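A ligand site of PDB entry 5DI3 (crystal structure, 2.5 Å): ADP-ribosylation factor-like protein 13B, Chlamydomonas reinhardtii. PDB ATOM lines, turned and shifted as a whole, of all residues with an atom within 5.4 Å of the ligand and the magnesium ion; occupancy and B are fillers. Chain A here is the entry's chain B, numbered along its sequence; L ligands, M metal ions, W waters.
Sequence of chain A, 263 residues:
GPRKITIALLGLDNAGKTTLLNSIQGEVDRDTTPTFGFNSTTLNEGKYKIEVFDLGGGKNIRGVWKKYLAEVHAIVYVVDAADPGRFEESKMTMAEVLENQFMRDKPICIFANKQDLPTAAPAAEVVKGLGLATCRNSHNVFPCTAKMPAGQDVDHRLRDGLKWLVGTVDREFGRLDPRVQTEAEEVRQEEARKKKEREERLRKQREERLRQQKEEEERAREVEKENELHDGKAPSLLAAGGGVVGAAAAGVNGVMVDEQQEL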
ATOM      1  N   GLY A  11     -13.564  -3.808   7.545  1.00  0.00           N
ATOM      2  CA  GLY A  11     -13.932  -3.993   8.939  1.00  0.00           C
ATOM      3  C   GLY A  11     -13.630  -2.724   9.715  1.00  0.00           C
ATOM      4  O   GLY A  11     -12.753  -1.950   9.322  1.00  0.00           O
ATOM      5  N   LEU A  12     -14.355  -2.510  10.813  1.00  0.00           N
ATOM      6  CA  LEU A  12     -14.181  -1.292  11.606  1.00  0.00           C
ATOM      7  C   LEU A  12     -12.749  -1.151  12.096  1.00  0.00           C
ATOM      8  O   LEU A  12     -12.010  -2.127  12.173  1.00  0.00           O
ATOM      9  CB  LEU A  12     -15.143  -1.279  12.808  1.00  0.00           C
ATOM     10  CG  LEU A  12     -16.628  -1.599  12.624  1.00  0.00           C
ATOM     11  CD1 LEU A  12     -17.342  -1.487  13.957  1.00  0.00           C
ATOM     12  CD2 LEU A  12     -17.269  -0.691  11.592  1.00  0.00           C
ATOM     13  N   ASP A  13     -12.374   0.080  12.431  1.00  0.00           N
ATOM     14  CA  ASP A  13     -11.088   0.339  13.073  1.00  0.00           C
ATOM     15  C   ASP A  13     -10.986  -0.475  14.373  1.00  0.00           C
ATOM     16  O   ASP A  13     -12.014  -0.779  14.995  1.00  0.00           O
ATOM     17  CB  ASP A  13     -10.915   1.826  13.373  1.00  0.00           C
ATOM     18  CG  ASP A  13     -11.972   2.365  14.320  1.00  0.00           C
ATOM     19  OD1 ASP A  13     -13.094   2.688  13.857  1.00  0.00           O
ATOM     20  OD2 ASP A  13     -11.683   2.467  15.536  1.00  0.00           O
ATOM     21  N   ASN A  14      -9.759  -0.841  14.735  1.00  0.00           N
ATOM     22  CA  ASN A  14      -9.451  -1.600  15.943  1.00  0.00           C
ATOM     23  C   ASN A  14      -9.869  -3.083  15.857  1.00  0.00           C
ATOM     24  O   ASN A  14      -9.663  -3.851  16.796  1.00  0.00           O
ATOM     25  CB  ASN A  14     -10.097  -0.935  17.177  1.00  0.00           C
ATOM     26  CG  ASN A  14      -9.508  -1.425  18.495  1.00  0.00           C
ATOM     27  OD1 ASN A  14      -8.341  -1.183  18.804  1.00  0.00           O
ATOM     28  ND2 ASN A  14     -10.341  -2.096  19.287  1.00  0.00           N
ATOM     29  N   ALA A  15     -10.433  -3.491  14.719  1.00  0.00           N
ATOM     30  CA  ALA A  15     -10.775  -4.894  14.519  1.00  0.00           C
ATOM     31  C   ALA A  15      -9.521  -5.771  14.426  1.00  0.00           C
ATOM     32  O   ALA A  15      -9.528  -6.917  14.883  1.00  0.00           O
ATOM     33  CB  ALA A  15     -11.645  -5.065  13.285  1.00  0.00           C
ATOM     34  N   GLY A  16      -8.463  -5.231  13.821  1.00  0.00           N
ATOM     35  CA  GLY A  16      -7.182  -5.927  13.758  1.00  0.00           C
ATOM     36  C   GLY A  16      -6.737  -6.309  12.356  1.00  0.00           C
ATOM     37  O   GLY A  16      -6.015  -7.296  12.167  1.00  0.00           O
ATOM     38  N   LYS A  17      -7.166  -5.532  11.362  1.00  0.00           N
ATOM     39  CA  LYS A  17      -6.869  -5.823   9.958  1.00  0.00           C
ATOM     40  C   LYS A  17      -5.364  -5.841   9.670  1.00  0.00           C
ATOM     41  O   LYS A  17      -4.846  -6.812   9.108  1.00  0.00           O
ATOM     42  CB  LYS A  17      -7.556  -4.789   9.059  1.00  0.00           C
ATOM     43  CG  LYS A  17      -9.054  -4.824   9.100  1.00  0.00           C
ATOM     44  CD  LYS A  17      -9.647  -3.729   8.212  1.00  0.00           C
ATOM     45  CE  LYS A  17      -9.284  -2.349   8.708  1.00  0.00           C
ATOM     46  NZ  LYS A  17     -10.126  -1.915   9.862  1.00  0.00           N
ATOM     47  N   THR A  18      -4.663  -4.765  10.046  1.00  0.00           N
ATOM     48  CA  THR A  18      -3.235  -4.636   9.747  1.00  0.00           C
ATOM     49  C   THR A  18      -2.422  -5.693  10.473  1.00  0.00           C
ATOM     50  O   THR A  18      -1.506  -6.298   9.904  1.00  0.00           O
ATOM     51  CB  THR A  18      -2.694  -3.230  10.129  1.00  0.00           C
ATOM     52  OG1 THR A  18      -3.393  -2.227   9.372  1.00  0.00           O
ATOM     53  CG2 THR A  18      -1.213  -3.132   9.833  1.00  0.00           C
ATOM     54  N   THR A  19      -2.758  -5.913  11.742  1.00  0.00           N
ATOM     55  CA  THR A  19      -2.053  -6.893  12.574  1.00  0.00           C
ATOM     56  C   THR A  19      -2.185  -8.293  11.985  1.00  0.00           C
ATOM     57  O   THR A  19      -1.231  -9.058  11.957  1.00  0.00           O
ATOM     58  CB  THR A  19      -2.606  -6.886  14.007  1.00  0.00           C
ATOM     59  OG1 THR A  19      -2.640  -5.542  14.501  1.00  0.00           O
ATOM     60  CG2 THR A  19      -1.766  -7.761  14.930  1.00  0.00           C
ATOM     61  N   LEU A  20      -3.387  -8.615  11.531  1.00  0.00           N
ATOM     62  CA  LEU A  20      -3.655  -9.907  10.913  1.00  0.00           C
ATOM     63  C   LEU A  20      -2.832 -10.021   9.629  1.00  0.00           C
ATOM     64  O   LEU A  20      -2.255 -11.071   9.335  1.00  0.00           O
ATOM     65  CB  LEU A  20      -5.152 -10.065  10.632  1.00  0.00           C
ATOM     66  CG  LEU A  20      -5.702 -11.401  10.103  1.00  0.00           C
ATOM     67  CD1 LEU A  20      -7.099 -11.667  10.687  1.00  0.00           C
ATOM     68  CD2 LEU A  20      -5.744 -11.403   8.586  1.00  0.00           C
ATOM     69  N   ASP A  31       4.443  -3.751  15.655  1.00  0.00           N
ATOM     70  CA  ASP A  31       3.233  -3.206  16.256  1.00  0.00           C
ATOM     71  C   ASP A  31       2.615  -2.219  15.291  1.00  0.00           C
ATOM     72  O   ASP A  31       3.225  -1.870  14.271  1.00  0.00           O
ATOM     73  CB  ASP A  31       3.482  -2.567  17.609  1.00  0.00           C
ATOM     74  CG  ASP A  31       2.267  -2.675  18.531  1.00  0.00           C
ATOM     75  OD1 ASP A  31       1.141  -2.873  18.013  1.00  0.00           O
ATOM     76  OD2 ASP A  31       2.440  -2.565  19.765  1.00  0.00           O
ATOM     77  N   THR A  32       1.406  -1.768  15.603  1.00  0.00           N
ATOM     78  CA  THR A  32       0.577  -1.114  14.602  1.00  0.00           C
ATOM     79  C   THR A  32      -0.018   0.212  15.062  1.00  0.00           C
ATOM     80  O   THR A  32      -0.318   0.401  16.228  1.00  0.00           O
ATOM     81  CB  THR A  32      -0.577  -2.045  14.158  1.00  0.00           C
ATOM     82  OG1 THR A  32      -1.212  -2.592  15.325  1.00  0.00           O
ATOM     83  CG2 THR A  32      -0.053  -3.188  13.288  1.00  0.00           C
ATOM     84  N   THR A  33      -0.191   1.122  14.103  1.00  0.00           N
ATOM     85  CA  THR A  33      -0.873   2.379  14.320  1.00  0.00           C
ATOM     86  C   THR A  33      -2.116   2.357  13.447  1.00  0.00           C
ATOM     87  O   THR A  33      -2.159   1.592  12.487  1.00  0.00           O
ATOM     88  CB  THR A  33       0.011   3.581  13.946  1.00  0.00           C
ATOM     89  OG1 THR A  33       0.186   3.620  12.528  1.00  0.00           O
ATOM     90  CG2 THR A  33       1.374   3.454  14.621  1.00  0.00           C
ATOM     91  N   PRO A  34      -3.128   3.173  13.773  1.00  0.00           N
ATOM     92  CA  PRO A  34      -4.330   3.239  12.923  1.00  0.00           C
ATOM     93  C   PRO A  34      -3.992   3.487  11.449  1.00  0.00           C
ATOM     94  O   PRO A  34      -2.992   4.153  11.152  1.00  0.00           O
ATOM     95  CB  PRO A  34      -5.109   4.427  13.503  1.00  0.00           C
ATOM     96  CG  PRO A  34      -4.707   4.462  14.946  1.00  0.00           C
ATOM     97  CD  PRO A  34      -3.258   4.027  14.972  1.00  0.00           C
ATOM     98  N   THR A  35      -4.794   2.940  10.539  1.00  0.00           N
ATOM     99  CA  THR A  35      -4.578   3.146   9.104  1.00  0.00           C
ATOM    100  C   THR A  35      -5.527   4.204   8.570  1.00  0.00           C
ATOM    101  O   THR A  35      -6.745   4.126   8.768  1.00  0.00           O
ATOM    102  CB  THR A  35      -4.768   1.840   8.300  1.00  0.00           C
ATOM    103  OG1 THR A  35      -3.913   0.812   8.837  1.00  0.00           O
ATOM    104  CG2 THR A  35      -4.430   2.058   6.829  1.00  0.00           C
ATOM    105  N   ASP A  54      -4.769  -3.065   2.198  1.00  0.00           N
ATOM    106  CA  ASP A  54      -5.026  -2.819   3.619  1.00  0.00           C
ATOM    107  C   ASP A  54      -5.527  -1.389   3.793  1.00  0.00           C
ATOM    108  O   ASP A  54      -4.791  -0.427   3.570  1.00  0.00           O
ATOM    109  CB  ASP A  54      -3.767  -3.054   4.458  1.00  0.00           C
ATOM    110  CG  ASP A  54      -3.995  -2.779   5.937  1.00  0.00           C
ATOM    111  OD1 ASP A  54      -5.163  -2.672   6.365  1.00  0.00           O
ATOM    112  OD2 ASP A  54      -2.997  -2.663   6.691  1.00  0.00           O
ATOM    113  N   LEU A  55      -6.782  -1.259   4.208  1.00  0.00           N
ATOM    114  CA  LEU A  55      -7.413   0.045   4.316  1.00  0.00           C
ATOM    115  C   LEU A  55      -7.815   0.349   5.751  1.00  0.00           C
ATOM    116  O   LEU A  55      -7.875  -0.541   6.586  1.00  0.00           O
ATOM    117  CB  LEU A  55      -8.639   0.123   3.413  1.00  0.00           C
ATOM    118  CG  LEU A  55      -8.345  -0.060   1.917  1.00  0.00           C
ATOM    119  CD1 LEU A  55      -9.565   0.266   1.086  1.00  0.00           C
ATOM    120  CD2 LEU A  55      -7.163   0.777   1.484  1.00  0.00           C
ATOM    121  N   GLY A  56      -8.075   1.631   6.022  1.00  0.00           N
ATOM    122  CA  GLY A  56      -8.536   2.044   7.330  1.00  0.00           C
ATOM    123  C   GLY A  56     -10.038   1.879   7.446  1.00  0.00           C
ATOM    124  O   GLY A  56     -10.773   1.917   6.455  1.00  0.00           O
ATOM    125  N   GLY A  57     -10.507   1.686   8.679  1.00  0.00           N
ATOM    126  CA  GLY A  57     -11.922   1.498   8.916  1.00  0.00           C
ATOM    127  C   GLY A  57     -12.517   2.511   9.856  1.00  0.00           C
ATOM    128  O   GLY A  57     -13.665   2.371  10.295  1.00  0.00           O
ATOM    129  N   GLY A  58     -11.738   3.546  10.179  1.00  0.00           N
ATOM    130  CA  GLY A  58     -12.227   4.620  11.027  1.00  0.00           C
ATOM    131  C   GLY A  58     -13.344   5.372  10.318  1.00  0.00           C
ATOM    132  O   GLY A  58     -13.393   5.392   9.087  1.00  0.00           O
ATOM    133  N   ASN A 113     -11.856 -11.991  15.279  1.00  0.00           N
ATOM    134  CA  ASN A 113     -10.515 -11.809  15.815  1.00  0.00           C
ATOM    135  C   ASN A 113     -10.524 -11.509  17.319  1.00  0.00           C
ATOM    136  O   ASN A 113     -11.559 -11.146  17.883  1.00  0.00           O
ATOM    137  CB  ASN A 113      -9.810 -10.695  15.034  1.00  0.00           C
ATOM    138  CG  ASN A 113      -8.367 -10.491  15.474  1.00  0.00           C
ATOM    139  OD1 ASN A 113      -7.660 -11.445  15.790  1.00  0.00           O
ATOM    140  ND2 ASN A 113      -7.918  -9.238  15.470  1.00  0.00           N
ATOM    141  N   LYS A 114      -9.349 -11.666  17.950  1.00  0.00           N
ATOM    142  CA  LYS A 114      -9.104 -11.395  19.364  1.00  0.00           C
ATOM    143  C   LYS A 114      -9.749 -12.456  20.253  1.00  0.00           C
ATOM    144  O   LYS A 114     -10.272 -12.168  21.320  1.00  0.00           O
ATOM    145  CB  LYS A 114      -9.588  -9.999  19.755  1.00  0.00           C
ATOM    146  CG  LYS A 114      -9.063  -8.893  18.838  1.00  0.00           C
ATOM    147  CD  LYS A 114      -9.151  -7.534  19.494  1.00  0.00           C
ATOM    148  CE  LYS A 114      -8.963  -6.427  18.465  1.00  0.00           C
ATOM    149  NZ  LYS A 114      -8.781  -5.084  19.103  1.00  0.00           N
ATOM    150  N   GLN A 115      -9.675 -13.695  19.783  1.00  0.00           N
ATOM    151  CA  GLN A 115     -10.167 -14.852  20.536  1.00  0.00           C
ATOM    152  C   GLN A 115      -9.369 -15.095  21.812  1.00  0.00           C
ATOM    153  O   GLN A 115      -9.748 -15.944  22.617  1.00  0.00           O
ATOM    154  CB  GLN A 115     -10.130 -16.111  19.664  1.00  0.00           C
ATOM    155  CG  GLN A 115     -11.238 -16.165  18.639  1.00  0.00           C
ATOM    156  CD  GLN A 115     -12.611 -16.190  19.270  1.00  0.00           C
ATOM    157  OE1 GLN A 115     -12.842 -16.888  20.257  1.00  0.00           O
ATOM    158  NE2 GLN A 115     -13.546 -15.431  18.710  1.00  0.00           N
ATOM    159  N   ASP A 116      -8.274 -14.369  21.994  1.00  0.00           N
ATOM    160  CA  ASP A 116      -7.468 -14.501  23.206  1.00  0.00           C
ATOM    161  C   ASP A 116      -8.157 -13.818  24.377  1.00  0.00           C
ATOM    162  O   ASP A 116      -8.017 -14.256  25.519  1.00  0.00           O
ATOM    163  CB  ASP A 116      -6.071 -13.919  22.994  1.00  0.00           C
ATOM    164  CG  ASP A 116      -6.100 -12.463  22.560  1.00  0.00           C
ATOM    165  OD1 ASP A 116      -6.738 -12.159  21.516  1.00  0.00           O
ATOM    166  OD2 ASP A 116      -5.491 -11.611  23.246  1.00  0.00           O
ATOM    167  N   LEU A 117      -8.913 -12.764  24.097  1.00  0.00           N
ATOM    168  CA  LEU A 117      -9.568 -11.969  25.142  1.00  0.00           C
ATOM    169  C   LEU A 117     -10.754 -12.697  25.773  1.00  0.00           C
ATOM    170  O   LEU A 117     -11.510 -13.368  25.076  1.00  0.00           O
ATOM    171  CB  LEU A 117     -10.018 -10.628  24.568  1.00  0.00           C
ATOM    172  CG  LEU A 117      -8.917  -9.685  24.082  1.00  0.00           C
ATOM    173  CD1 LEU A 117      -9.511  -8.409  23.524  1.00  0.00           C
ATOM    174  CD2 LEU A 117      -7.967  -9.379  25.225  1.00  0.00           C
ATOM    175  N   CYS A 144     -10.037 -16.333  15.340  1.00  0.00           N
ATOM    176  CA  CYS A 144      -8.583 -16.278  15.293  1.00  0.00           C
ATOM    177  C   CYS A 144      -8.019 -15.346  16.352  1.00  0.00           C
ATOM    178  O   CYS A 144      -8.731 -14.548  16.951  1.00  0.00           O
ATOM    179  CB  CYS A 144      -8.112 -15.819  13.905  1.00  0.00           C
ATOM    180  SG  CYS A 144      -8.715 -14.187  13.395  1.00  0.00           S
ATOM    181  N   THR A 145      -6.708 -15.461  16.566  1.00  0.00           N
ATOM    182  CA  THR A 145      -5.966 -14.517  17.386  1.00  0.00           C
ATOM    183  C   THR A 145      -4.831 -13.959  16.542  1.00  0.00           C
ATOM    184  O   THR A 145      -3.809 -14.622  16.325  1.00  0.00           O
ATOM    185  CB  THR A 145      -5.413 -15.192  18.659  1.00  0.00           C
ATOM    186  OG1 THR A 145      -6.504 -15.709  19.431  1.00  0.00           O
ATOM    187  CG2 THR A 145      -4.620 -14.186  19.495  1.00  0.00           C
ATOM    188  N   ALA A 146      -5.016 -12.750  16.041  1.00  0.00           N
ATOM    189  CA  ALA A 146      -4.034 -12.125  15.156  1.00  0.00           C
ATOM    190  C   ALA A 146      -2.764 -11.757  15.918  1.00  0.00           C
ATOM    191  O   ALA A 146      -1.672 -11.720  15.349  1.00  0.00           O
ATOM    192  CB  ALA A 146      -4.633 -10.917  14.474  1.00  0.00           C
ATOM    193  N   LYS A 147      -2.913 -11.467  17.208  1.00  0.00           N
ATOM    194  CA  LYS A 147      -1.776 -11.100  18.031  1.00  0.00           C
ATOM    195  C   LYS A 147      -1.464 -12.195  19.059  1.00  0.00           C
ATOM    196  O   LYS A 147      -1.824 -12.089  20.228  1.00  0.00           O
ATOM    197  CB  LYS A 147      -2.021  -9.759  18.735  1.00  0.00           C
ATOM    198  CG  LYS A 147      -0.760  -9.113  19.294  1.00  0.00           C
ATOM    199  CD  LYS A 147      -0.903  -7.603  19.431  1.00  0.00           C
ATOM    200  CE  LYS A 147      -1.047  -7.168  20.880  1.00  0.00           C
ATOM    201  NZ  LYS A 147      -1.032  -5.670  21.044  1.00  0.00           N
HETATM  202  P1  LIG L   1      -7.418   0.462  11.522  1.00  0.00           P
HETATM  203  O1  LIG L   1      -6.126   0.486  10.736  1.00  0.00           O
HETATM  204  O2  LIG L   1      -8.667   0.162  10.724  1.00  0.00           O
HETATM  205  O3  LIG L   1      -7.496   1.782  12.250  1.00  0.00           O
HETATM  206  N1  LIG L   1      -7.282  -0.645  12.658  1.00  0.00           N
HETATM  207  P2  LIG L   1      -6.893  -2.161  12.392  1.00  0.00           P
HETATM  208  O4  LIG L   1      -5.792  -2.270  11.396  1.00  0.00           O
HETATM  209  O5  LIG L   1      -8.156  -2.880  12.060  1.00  0.00           O
HETATM  210  O6  LIG L   1      -6.412  -2.725  13.736  1.00  0.00           O
HETATM  211  P3  LIG L   1      -4.953  -2.928  14.155  1.00  0.00           P
HETATM  212  O7  LIG L   1      -4.245  -1.621  14.095  1.00  0.00           O
HETATM  213  O8  LIG L   1      -4.328  -4.064  13.445  1.00  0.00           O
HETATM  214  O9  LIG L   1      -5.007  -3.343  15.681  1.00  0.00           O
HETATM  215  C1  LIG L   1      -5.819  -2.658  16.615  1.00  0.00           C
HETATM  216  C2  LIG L   1      -5.407  -3.024  18.034  1.00  0.00           C
HETATM  217  O10 LIG L   1      -5.877  -4.358  18.367  1.00  0.00           O
HETATM  218  C3  LIG L   1      -3.902  -3.040  18.273  1.00  0.00           C
HETATM  219  O11 LIG L   1      -3.616  -2.517  19.568  1.00  0.00           O
HETATM  220  C4  LIG L   1      -3.561  -4.517  18.171  1.00  0.00           C
HETATM  221  O12 LIG L   1      -2.362  -4.820  18.850  1.00  0.00           O
HETATM  222  C5  LIG L   1      -4.792  -5.149  18.829  1.00  0.00           C
HETATM  223  N2  LIG L   1      -5.041  -6.536  18.411  1.00  0.00           N
HETATM  224  C6  LIG L   1      -5.084  -6.986  17.115  1.00  0.00           C
HETATM  225  N3  LIG L   1      -5.323  -8.264  17.007  1.00  0.00           N
HETATM  226  C7  LIG L   1      -5.447  -8.692  18.316  1.00  0.00           C
HETATM  227  C8  LIG L   1      -5.714  -9.997  18.821  1.00  0.00           C
HETATM  228  O13 LIG L   1      -5.890 -11.046  18.183  1.00  0.00           O
HETATM  229  N4  LIG L   1      -5.776 -10.013  20.205  1.00  0.00           N
HETATM  230  C9  LIG L   1      -5.589  -8.915  21.015  1.00  0.00           C
HETATM  231  N5  LIG L   1      -5.683  -9.151  22.327  1.00  0.00           N
HETATM  232  N6  LIG L   1      -5.345  -7.689  20.552  1.00  0.00           N
HETATM  233  C10 LIG L   1      -5.282  -7.644  19.201  1.00  0.00           C
HETATM  234 MG    MG M   1      -4.908  -0.967   9.904  1.00  0.00          MG
HETATM  235  O   HOH W   1      -7.639   1.591  15.184  1.00  0.00           O
HETATM  236  O   HOH W   2      -3.833  -0.514  11.773  1.00  0.00           O
HETATM  237  O   HOH W   3      -8.650   3.966  10.743  1.00  0.00           O
HETATM  238  O   HOH W   4      -6.038  -1.284   8.352  1.00  0.00           O
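Water W2 bridges O7 of the ligand and O of Thr 33. Water W4 bridges OD1 of Asp 54 (2.6 Å) and O of Leu 55 (2.7 Å). Water W3 lies within hydrogen-bond range of the backbone carbonyl oxygen (O) of Thr 35, an oxygen (O3) of the ligand and the backbone NH (N) of Gly 58. Water W1 bridges an oxygen (O3) of the ligand and the backbone NH of Asn 14.
Asp 54 touches the magnesium ion (OD1 to MG, 3.9 Å). Within 4 Å of the magnesium ion: Thr 18, Thr 35 and Asp 54.
OG1 of Thr 18 lies close to OD2 of Asp 54, at 2.7 Å. The side-chain hydroxyl (OG1) of Thr 19 lies within hydrogen-bond range of the side-chain hydroxyl (OG1) of Thr 32. N of Asp 116 sits at hydrogen-bond distance from OG1 of Thr 145, 3.4 Å away. NZ of Lys 17 lies within hydrogen-bond range of O of Leu 12, at 3.0 Å. The side-chain amide oxygen (OD1) of Asn 113 lies within hydrogen-bond range of the backbone NH (N) of Ala 146 (3.0 Å). OD1 of Asn 113 lies close to O of Cys 144. NZ of Lys 114 lies within hydrogen-bond range of O of Asn 14 (2.8 Å). The backbone carbonyl oxygen (O) of Gly 57 lies within hydrogen-bond range of the backbone NH (N) of Asp 13, 3.4 Å away.
The backbone NH of Asn 14 sits close to a nitrogen (N1) of the ligand, 3.2 Å away. Leu 12 touches the ligand (O to O5, 3.9 Å). Asp 13 touches the ligand. Ala 15 touches the ligand. Pro 34 touches the ligand. Gly 56 touches the ligand. Leu 117 touches the ligand. Thr 145 touches the ligand (C to O13, 3.5 Å). Hydrophobic or aromatic side chains within 4 Å of the ligand: Pro 34, Leu 117 and Ala 146. 20 residues have an atom within 4 Å of the ligand: Leu 12, Asp 13, Asn 14, Ala 15, Gly 16, Lys 17, Thr 18, Thr 19, Thr 32, Pro 34, Thr 35, Gly 56, Gly 57, Asn 113, Lys 114, Asp 116, Leu 117, Thr 145, Ala 146 and Lys 147. The nearest printed residue that does not touch the ligand is Asp 31 (4.1 Å).
The magnesium ion is bound by water W4 (1.9 Å), OG1 of Thr 18 (2.0 Å), O1 of the ligand (2.1 Å), O4 of the ligand (2.2 Å), water W2 (2.2 Å) and OG1 of Thr 35 (2.3 Å).
The backbone NH (N) of Thr 18 lies within hydrogen-bond range of an oxygen (O8) of the ligand, at 3.5 Å. The backbone NH (N) of Thr 35 sits at hydrogen-bond distance from an oxygen (O3) of the ligand (3.4 Å). The backbone NH (N) of Thr 19 is in hydrogen-bond range of an oxygen (O8) of the ligand (3.0 Å). OG1 of Thr 19 is in hydrogen-bond range of O8 of the ligand (2.5 Å). The side-chain carboxylate (OD2) of Asp 116 lies within hydrogen-bond range of a nitrogen (N5) of the ligand (2.6 Å). The backbone NH (N) of Lys 17 lies within hydrogen-bond range of an oxygen (O5) of the ligand (2.9 Å). The side-chain amino group of Lys 17 lies within salt-bridge range of an oxygen (O2) of the ligand. O13 of the ligand sits at hydrogen-bond distance from N of Lys 147 (3.2 Å). An oxygen (O12) of the ligand sits at hydrogen-bond distance from the side-chain amino group (NZ) of Lys 147 (2.7 Å). The backbone NH (N) of Ala 146 is in hydrogen-bond range of an oxygen (O13) of the ligand, at 2.9 Å. N of Gly 16 lies within hydrogen-bond range of O5 of the ligand, 3.0 Å away. The side-chain amide oxygen (OD1) of Asn 113 sits close to an oxygen (O13) of the ligand (3.0 Å). An oxygen (O10) of the ligand is in hydrogen-bond range of the side-chain amino group (NZ) of Lys 114, 3.1 Å away. An oxygen (O2) of the ligand is in hydrogen-bond range of the backbone NH of Gly 57 (3.1 Å). The side-chain hydroxyl (OG1) of Thr 32 is in hydrogen-bond range of an oxygen (O7) of the ligand (3.4 Å).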
